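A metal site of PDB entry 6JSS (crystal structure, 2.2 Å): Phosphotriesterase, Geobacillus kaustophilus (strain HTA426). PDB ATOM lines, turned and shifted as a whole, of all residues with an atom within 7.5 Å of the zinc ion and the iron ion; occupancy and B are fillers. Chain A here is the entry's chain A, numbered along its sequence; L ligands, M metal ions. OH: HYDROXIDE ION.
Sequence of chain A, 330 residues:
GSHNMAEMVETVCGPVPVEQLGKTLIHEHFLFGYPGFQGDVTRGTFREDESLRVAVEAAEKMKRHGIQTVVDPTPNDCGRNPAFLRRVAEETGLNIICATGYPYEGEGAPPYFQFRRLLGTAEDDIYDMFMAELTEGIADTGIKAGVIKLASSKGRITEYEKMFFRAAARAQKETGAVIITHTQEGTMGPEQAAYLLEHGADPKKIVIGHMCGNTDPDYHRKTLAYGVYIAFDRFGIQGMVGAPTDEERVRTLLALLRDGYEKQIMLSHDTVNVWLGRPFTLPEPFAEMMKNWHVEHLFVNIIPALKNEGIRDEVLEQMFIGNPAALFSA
A ring nitrogen (NE2) of His 210 binds the zinc ion, 2.0 Å away.
The zinc ion is bound by OQ1 of KCX 149, 2.1 Å away.
O of the ligand binds the zinc ion, at 2.1 Å.
ND1 of His 182 is bound to the zinc ion, 2.1 Å away.
The zinc ion has four donor atoms within binding distance.
OG1 of Thr 74 is in hydrogen-bond range of ND1 of His 29.
A ring nitrogen (NE2) of His 182 is in hydrogen-bond range of the side-chain amide oxygen (OE1) of Gln 184 (2.8 Å).
The side-chain carboxylate (OD1) of Asp 233 is in hydrogen-bond range of a ring nitrogen (ND1) of His 210 (2.9 Å).
N of Asp 270 lies within hydrogen-bond range of O of Asp 233, 3.0 Å away.
The backbone carbonyl oxygen (O) of Leu 150 is in hydrogen-bond range of the backbone NH (N) of His 182 (2.7 Å).
OD2 of Asp 270 is in salt-bridge range of NE of Arg 234 (2.7 Å).
O of His 210 sits at hydrogen-bond distance from OG1 of Thr 183 (3.1 Å).
N of His 29 sits at hydrogen-bond distance from O of Thr 271.
Within 4 Å of the iron ion: His 27, His 29, KCX 149 and Asp 270.
The nearest printed residue that does not touch the iron ion is His 210 (4.2 Å).
The iron ion is bound by a ring nitrogen (NE2) of His 27, OQ2 of KCX 149, an oxygen (O) of the ligand, the side-chain carboxylate (OD1) of Asp 270 and a ring nitrogen (NE2) of His 29.
Residues that only touch the zinc ion: Arg 234 (3.8 Å).
Of the 25 residues printed, 4 come within 4 Å of the zinc ion.
The nearest printed residue that does not touch the zinc ion is His 27 (4.1 Å).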
ATOM      1  N   HIS A  27      31.664 -20.097  24.614  1.00  0.00           N
ATOM      2  CA  HIS A  27      30.361 -20.655  25.088  1.00  0.00           C
ATOM      3  C   HIS A  27      29.152 -19.949  24.478  1.00  0.00           C
ATOM      4  O   HIS A  27      28.767 -18.943  24.981  1.00  0.00           O
ATOM      5  CB  HIS A  27      30.302 -20.610  26.620  1.00  0.00           C
ATOM      6  CG  HIS A  27      29.207 -21.391  27.256  1.00  0.00           C
ATOM      7  ND1 HIS A  27      29.446 -22.271  28.228  1.00  0.00           N
ATOM      8  CD2 HIS A  27      27.887 -21.398  27.068  1.00  0.00           C
ATOM      9  CE1 HIS A  27      28.342 -22.807  28.630  1.00  0.00           C
ATOM     10  NE2 HIS A  27      27.364 -22.289  27.954  1.00  0.00           N
ATOM     11  N   GLU A  28      28.609 -20.512  23.391  1.00  0.00           N
ATOM     12  CA  GLU A  28      27.431 -19.929  22.701  1.00  0.00           C
ATOM     13  C   GLU A  28      26.525 -21.071  22.217  1.00  0.00           C
ATOM     14  O   GLU A  28      27.065 -22.103  21.778  1.00  0.00           O
ATOM     15  CB  GLU A  28      27.874 -19.044  21.541  1.00  0.00           C
ATOM     16  CG  GLU A  28      28.825 -17.935  21.945  1.00  0.00           C
ATOM     17  CD  GLU A  28      28.192 -16.846  22.803  1.00  0.00           C
ATOM     18  OE1 GLU A  28      26.952 -16.742  22.798  1.00  0.00           O
ATOM     19  OE2 GLU A  28      28.950 -16.105  23.464  1.00  0.00           O
ATOM     20  N   HIS A  29      25.203 -20.874  22.289  1.00  0.00           N
ATOM     21  CA  HIS A  29      24.243 -21.906  21.864  1.00  0.00           C
ATOM     22  C   HIS A  29      23.475 -21.488  20.607  1.00  0.00           C
ATOM     23  O   HIS A  29      22.675 -20.619  20.694  1.00  0.00           O
ATOM     24  CB  HIS A  29      23.286 -22.239  22.989  1.00  0.00           C
ATOM     25  CG  HIS A  29      23.932 -22.810  24.197  1.00  0.00           C
ATOM     26  ND1 HIS A  29      24.187 -24.118  24.343  1.00  0.00           N
ATOM     27  CD2 HIS A  29      24.333 -22.233  25.322  1.00  0.00           C
ATOM     28  CE1 HIS A  29      24.733 -24.324  25.497  1.00  0.00           C
ATOM     29  NE2 HIS A  29      24.832 -23.201  26.098  1.00  0.00           N
ATOM     30  N   PHE A  32      19.005 -24.311  21.646  1.00  0.00           N
ATOM     31  CA  PHE A  32      18.946 -24.810  23.008  1.00  0.00           C
ATOM     32  C   PHE A  32      17.487 -24.988  23.410  1.00  0.00           C
ATOM     33  O   PHE A  32      16.645 -24.158  23.081  1.00  0.00           O
ATOM     34  CB  PHE A  32      19.645 -23.884  24.003  1.00  0.00           C
ATOM     35  CG  PHE A  32      19.471 -24.313  25.438  1.00  0.00           C
ATOM     36  CD1 PHE A  32      20.353 -25.222  26.025  1.00  0.00           C
ATOM     37  CD2 PHE A  32      18.401 -23.849  26.188  1.00  0.00           C
ATOM     38  CE1 PHE A  32      20.173 -25.629  27.349  1.00  0.00           C
ATOM     39  CE2 PHE A  32      18.221 -24.255  27.511  1.00  0.00           C
ATOM     40  CZ  PHE A  32      19.110 -25.136  28.087  1.00  0.00           C
ATOM     41  N   ASP A  72      30.139 -24.539  21.107  1.00  0.00           N
ATOM     42  CA  ASP A  72      28.729 -24.679  21.426  1.00  0.00           C
ATOM     43  C   ASP A  72      28.581 -25.869  22.354  1.00  0.00           C
ATOM     44  O   ASP A  72      28.572 -27.028  21.897  1.00  0.00           O
ATOM     45  CB  ASP A  72      27.898 -24.875  20.145  1.00  0.00           C
ATOM     46  CG  ASP A  72      26.401 -24.864  20.408  1.00  0.00           C
ATOM     47  OD1 ASP A  72      25.979 -25.360  21.462  1.00  0.00           O
ATOM     48  OD2 ASP A  72      25.645 -24.351  19.544  1.00  0.00           O
ATOM     49  N   PRO A  73      28.464 -25.652  23.642  1.00  0.00           N
ATOM     50  CA  PRO A  73      28.455 -26.777  24.576  1.00  0.00           C
ATOM     51  C   PRO A  73      27.044 -27.212  24.950  1.00  0.00           C
ATOM     52  O   PRO A  73      26.786 -27.524  26.120  1.00  0.00           O
ATOM     53  CB  PRO A  73      29.208 -26.221  25.783  1.00  0.00           C
ATOM     54  CG  PRO A  73      28.792 -24.770  25.783  1.00  0.00           C
ATOM     55  CD  PRO A  73      28.515 -24.364  24.329  1.00  0.00           C
ATOM     56  N   THR A  74      26.126 -27.216  23.987  1.00  0.00           N
ATOM     57  CA  THR A  74      24.758 -27.624  24.271  1.00  0.00           C
ATOM     58  C   THR A  74      24.715 -29.080  24.735  1.00  0.00           C
ATOM     59  O   THR A  74      25.192 -29.958  24.005  1.00  0.00           O
ATOM     60  CB  THR A  74      23.896 -27.460  23.024  1.00  0.00           C
ATOM     61  OG1 THR A  74      23.820 -26.077  22.690  1.00  0.00           O
ATOM     62  CG2 THR A  74      22.498 -28.005  23.279  1.00  0.00           C
ATOM     63  N   PRO A  75      24.180 -29.375  25.919  1.00  0.00           N
ATOM     64  CA  PRO A  75      24.121 -30.759  26.386  1.00  0.00           C
ATOM     65  C   PRO A  75      23.328 -31.658  25.449  1.00  0.00           C
ATOM     66  O   PRO A  75      22.509 -31.198  24.643  1.00  0.00           O
ATOM     67  CB  PRO A  75      23.425 -30.653  27.753  1.00  0.00           C
ATOM     68  CG  PRO A  75      23.724 -29.226  28.201  1.00  0.00           C
ATOM     69  CD  PRO A  75      23.703 -28.417  26.944  1.00  0.00           C
ATOM     70  N   TYR A 104      23.054 -30.158  34.644  1.00  0.00           N
ATOM     71  CA  TYR A 104      22.981 -30.421  36.089  1.00  0.00           C
ATOM     72  C   TYR A 104      21.563 -30.824  36.479  1.00  0.00           C
ATOM     73  O   TYR A 104      20.600 -30.621  35.732  1.00  0.00           O
ATOM     74  CB  TYR A 104      23.457 -29.213  36.913  1.00  0.00           C
ATOM     75  CG  TYR A 104      22.516 -28.016  36.923  1.00  0.00           C
ATOM     76  CD1 TYR A 104      22.461 -27.105  35.864  1.00  0.00           C
ATOM     77  CD2 TYR A 104      21.680 -27.776  38.007  1.00  0.00           C
ATOM     78  CE1 TYR A 104      21.600 -26.015  35.886  1.00  0.00           C
ATOM     79  CE2 TYR A 104      20.834 -26.703  38.046  1.00  0.00           C
ATOM     80  CZ  TYR A 104      20.780 -25.831  36.994  1.00  0.00           C
ATOM     81  OH  TYR A 104      19.905 -24.772  37.078  1.00  0.00           O
ATOM     82  N   GLU A 107      18.173 -28.487  36.207  1.00  0.00           N
ATOM     83  CA  GLU A 107      17.722 -27.988  34.907  1.00  0.00           C
ATOM     84  C   GLU A 107      17.947 -29.049  33.836  1.00  0.00           C
ATOM     85  O   GLU A 107      18.297 -28.752  32.691  1.00  0.00           O
ATOM     86  CB  GLU A 107      18.396 -26.663  34.554  1.00  0.00           C
ATOM     87  CG  GLU A 107      17.480 -25.443  34.761  1.00  0.00           C
ATOM     88  CD  GLU A 107      18.213 -24.105  34.730  1.00  0.00           C
ATOM     89  OE1 GLU A 107      17.651 -23.112  35.239  1.00  0.00           O
ATOM     90  OE2 GLU A 107      19.345 -24.047  34.191  1.00  0.00           O
ATOM     91  N   KCX A 149      31.192 -31.544  28.246  1.00  0.00           N
ATOM     92  CA  KCX A 149      30.456 -30.544  29.009  1.00  0.00           C
ATOM     93  CB  KCX A 149      29.219 -30.069  28.227  1.00  0.00           C
ATOM     94  CG  KCX A 149      28.307 -29.091  28.997  1.00  0.00           C
ATOM     95  CD  KCX A 149      29.107 -27.869  29.430  1.00  0.00           C
ATOM     96  CE  KCX A 149      28.209 -26.828  30.090  1.00  0.00           C
ATOM     97  NZ  KCX A 149      27.207 -26.282  29.093  1.00  0.00           N
ATOM     98  C   KCX A 149      30.032 -31.135  30.350  1.00  0.00           C
ATOM     99  O   KCX A 149      29.456 -32.222  30.408  1.00  0.00           O
ATOM    100  CX  KCX A 149      26.554 -25.164  29.387  1.00  0.00           C
ATOM    101  OQ1 KCX A 149      26.792 -24.597  30.474  1.00  0.00           O
ATOM    102  OQ2 KCX A 149      25.727 -24.693  28.585  1.00  0.00           O
ATOM    103  N   LEU A 150      30.360 -30.427  31.424  1.00  0.00           N
ATOM    104  CA  LEU A 150      29.988 -30.820  32.792  1.00  0.00           C
ATOM    105  C   LEU A 150      29.160 -29.754  33.477  1.00  0.00           C
ATOM    106  O   LEU A 150      29.355 -28.565  33.223  1.00  0.00           O
ATOM    107  CB  LEU A 150      31.240 -31.076  33.616  1.00  0.00           C
ATOM    108  CG  LEU A 150      31.996 -32.346  33.307  1.00  0.00           C
ATOM    109  CD1 LEU A 150      33.165 -32.449  34.270  1.00  0.00           C
ATOM    110  CD2 LEU A 150      31.046 -33.525  33.408  1.00  0.00           C
ATOM    111  N   ALA A 151      28.277 -30.130  34.395  1.00  0.00           N
ATOM    112  CA  ALA A 151      27.493 -29.121  35.091  1.00  0.00           C
ATOM    113  C   ALA A 151      27.240 -29.517  36.554  1.00  0.00           C
ATOM    114  O   ALA A 151      27.050 -30.688  36.855  1.00  0.00           O
ATOM    115  CB  ALA A 151      26.162 -28.900  34.377  1.00  0.00           C
ATOM    116  N   THR A 181      32.829 -26.464  31.795  1.00  0.00           N
ATOM    117  CA  THR A 181      31.842 -26.699  32.846  1.00  0.00           C
ATOM    118  C   THR A 181      30.844 -25.556  32.964  1.00  0.00           C
ATOM    119  O   THR A 181      31.080 -24.440  32.501  1.00  0.00           O
ATOM    120  CB  THR A 181      32.485 -26.938  34.223  1.00  0.00           C
ATOM    121  OG1 THR A 181      32.700 -25.676  34.853  1.00  0.00           O
ATOM    122  CG2 THR A 181      33.784 -27.678  34.117  1.00  0.00           C
ATOM    123  N   HIS A 182      29.731 -25.878  33.619  1.00  0.00           N
ATOM    124  CA  HIS A 182      28.685 -24.953  34.022  1.00  0.00           C
ATOM    125  C   HIS A 182      28.681 -24.887  35.551  1.00  0.00           C
ATOM    126  O   HIS A 182      28.667 -25.925  36.207  1.00  0.00           O
ATOM    127  CB  HIS A 182      27.332 -25.453  33.489  1.00  0.00           C
ATOM    128  CG  HIS A 182      26.127 -24.856  34.136  1.00  0.00           C
ATOM    129  ND1 HIS A 182      25.167 -24.163  33.411  1.00  0.00           N
ATOM    130  CD2 HIS A 182      25.677 -24.891  35.416  1.00  0.00           C
ATOM    131  CE1 HIS A 182      24.197 -23.777  34.232  1.00  0.00           C
ATOM    132  NE2 HIS A 182      24.486 -24.210  35.455  1.00  0.00           N
ATOM    133  N   THR A 183      28.729 -23.669  36.114  1.00  0.00           N
ATOM    134  CA  THR A 183      28.498 -23.491  37.550  1.00  0.00           C
ATOM    135  C   THR A 183      27.169 -22.786  37.761  1.00  0.00           C
ATOM    136  O   THR A 183      26.799 -21.894  37.000  1.00  0.00           O
ATOM    137  CB  THR A 183      29.621 -22.720  38.284  1.00  0.00           C
ATOM    138  OG1 THR A 183      29.819 -21.411  37.710  1.00  0.00           O
ATOM    139  CG2 THR A 183      30.920 -23.498  38.256  1.00  0.00           C
ATOM    140  N   GLN A 184      26.435 -23.212  38.783  1.00  0.00           N
ATOM    141  CA  GLN A 184      25.103 -22.686  39.016  1.00  0.00           C
ATOM    142  C   GLN A 184      25.174 -21.580  40.071  1.00  0.00           C
ATOM    143  O   GLN A 184      25.644 -21.826  41.180  1.00  0.00           O
ATOM    144  CB  GLN A 184      24.161 -23.822  39.441  1.00  0.00           C
ATOM    145  CG  GLN A 184      22.694 -23.442  39.537  1.00  0.00           C
ATOM    146  CD  GLN A 184      22.119 -22.820  38.265  1.00  0.00           C
ATOM    147  OE1 GLN A 184      22.656 -22.978  37.161  1.00  0.00           O
ATOM    148  NE2 GLN A 184      21.024 -22.097  38.428  1.00  0.00           N
ATOM    149  N   GLY A 209      33.176 -22.800  34.030  1.00  0.00           N
ATOM    150  CA  GLY A 209      32.243 -21.851  33.443  1.00  0.00           C
ATOM    151  C   GLY A 209      31.355 -21.151  34.437  1.00  0.00           C
ATOM    152  O   GLY A 209      31.339 -21.501  35.590  1.00  0.00           O
ATOM    153  N   HIS A 210      30.730 -20.102  33.926  1.00  0.00           N
ATOM    154  CA  HIS A 210      29.765 -19.213  34.594  1.00  0.00           C
ATOM    155  C   HIS A 210      30.432 -18.602  35.834  1.00  0.00           C
ATOM    156  O   HIS A 210      29.770 -18.455  36.822  1.00  0.00           O
ATOM    157  CB  HIS A 210      28.421 -19.937  34.801  1.00  0.00           C
ATOM    158  CG  HIS A 210      27.811 -20.629  33.619  1.00  0.00           C
ATOM    159  ND1 HIS A 210      27.869 -20.143  32.359  1.00  0.00           N
ATOM    160  CD2 HIS A 210      27.097 -21.773  33.526  1.00  0.00           C
ATOM    161  CE1 HIS A 210      27.235 -20.947  31.546  1.00  0.00           C
ATOM    162  NE2 HIS A 210      26.746 -21.950  32.237  1.00  0.00           N
ATOM    163  N   ASP A 233      31.328 -15.934  30.940  1.00  0.00           N
ATOM    164  CA  ASP A 233      30.686 -16.371  29.702  1.00  0.00           C
ATOM    165  C   ASP A 233      29.193 -16.054  29.665  1.00  0.00           C
ATOM    166  O   ASP A 233      28.504 -16.557  28.780  1.00  0.00           O
ATOM    167  CB  ASP A 233      30.922 -17.868  29.505  1.00  0.00           C
ATOM    168  CG  ASP A 233      30.547 -18.668  30.738  1.00  0.00           C
ATOM    169  OD1 ASP A 233      29.765 -18.148  31.549  1.00  0.00           O
ATOM    170  OD2 ASP A 233      31.038 -19.804  30.917  1.00  0.00           O
ATOM    171  N   ARG A 234      28.679 -15.219  30.566  1.00  0.00           N
ATOM    172  CA  ARG A 234      27.263 -14.869  30.532  1.00  0.00           C
ATOM    173  C   ARG A 234      27.037 -13.361  30.491  1.00  0.00           C
ATOM    174  O   ARG A 234      26.069 -12.845  31.048  1.00  0.00           O
ATOM    175  CB  ARG A 234      26.524 -15.484  31.707  1.00  0.00           C
ATOM    176  CG  ARG A 234      26.286 -16.971  31.506  1.00  0.00           C
ATOM    177  CD  ARG A 234      25.441 -17.557  32.624  1.00  0.00           C
ATOM    178  NE  ARG A 234      24.676 -18.705  32.144  1.00  0.00           N
ATOM    179  CZ  ARG A 234      23.882 -19.418  32.910  1.00  0.00           C
ATOM    180  NH1 ARG A 234      23.756 -19.101  34.189  1.00  0.00           N
ATOM    181  NH2 ARG A 234      23.221 -20.466  32.409  1.00  0.00           N
ATOM    182  N   HIS A 269      28.963 -15.010  25.959  1.00  0.00           N
ATOM    183  CA  HIS A 269      27.625 -14.590  26.345  1.00  0.00           C
ATOM    184  C   HIS A 269      26.690 -15.720  26.747  1.00  0.00           C
ATOM    185  O   HIS A 269      25.697 -15.438  27.427  1.00  0.00           O
ATOM    186  CB  HIS A 269      26.903 -13.855  25.223  1.00  0.00           C
ATOM    187  CG  HIS A 269      27.734 -12.888  24.459  1.00  0.00           C
ATOM    188  ND1 HIS A 269      28.481 -13.252  23.372  1.00  0.00           N
ATOM    189  CD2 HIS A 269      27.898 -11.544  24.602  1.00  0.00           C
ATOM    190  CE1 HIS A 269      29.079 -12.185  22.873  1.00  0.00           C
ATOM    191  NE2 HIS A 269      28.738 -11.131  23.606  1.00  0.00           N
ATOM    192  N   ASP A 270      26.931 -16.960  26.315  1.00  0.00           N
ATOM    193  CA  ASP A 270      25.998 -18.049  26.596  1.00  0.00           C
ATOM    194  C   ASP A 270      24.642 -17.747  25.948  1.00  0.00           C
ATOM    195  O   ASP A 270      23.583 -17.923  26.565  1.00  0.00           O
ATOM    196  CB  ASP A 270      25.880 -18.262  28.104  1.00  0.00           C
ATOM    197  CG  ASP A 270      25.297 -19.607  28.512  1.00  0.00           C
ATOM    198  OD1 ASP A 270      25.226 -20.561  27.698  1.00  0.00           O
ATOM    199  OD2 ASP A 270      24.935 -19.714  29.704  1.00  0.00           O
ATOM    200  N   THR A 271      24.657 -17.258  24.715  1.00  0.00           N
ATOM    201  CA  THR A 271      23.392 -16.924  24.071  1.00  0.00           C
ATOM    202  C   THR A 271      22.650 -18.187  23.688  1.00  0.00           C
ATOM    203  O   THR A 271      23.236 -19.256  23.522  1.00  0.00           O
ATOM    204  CB  THR A 271      23.604 -16.071  22.804  1.00  0.00           C
ATOM    205  OG1 THR A 271      24.482 -16.737  21.898  1.00  0.00           O
ATOM    206  CG2 THR A 271      24.182 -14.722  23.177  1.00  0.00           C
ATOM    207  N   VAL A 272      21.326 -18.068  23.594  1.00  0.00           N
ATOM    208  CA  VAL A 272      20.496 -19.046  22.920  1.00  0.00           C
ATOM    209  C   VAL A 272      19.911 -18.355  21.700  1.00  0.00           C
ATOM    210  O   VAL A 272      19.054 -17.473  21.813  1.00  0.00           O
ATOM    211  CB  VAL A 272      19.378 -19.595  23.804  1.00  0.00           C
ATOM    212  CG1 VAL A 272      18.537 -20.616  22.993  1.00  0.00           C
ATOM    213  CG2 VAL A 272      19.988 -20.210  25.055  1.00  0.00           C
HETATM  214  O    OH L   1      24.203 -22.475  30.023  1.00  0.00           O
HETATM  215 ZN    ZN M   1      25.502 -23.326  31.476  1.00  0.00          ZN
HETATM  216 FE    FE M   2      25.325 -22.667  28.199  1.00  0.00          FE
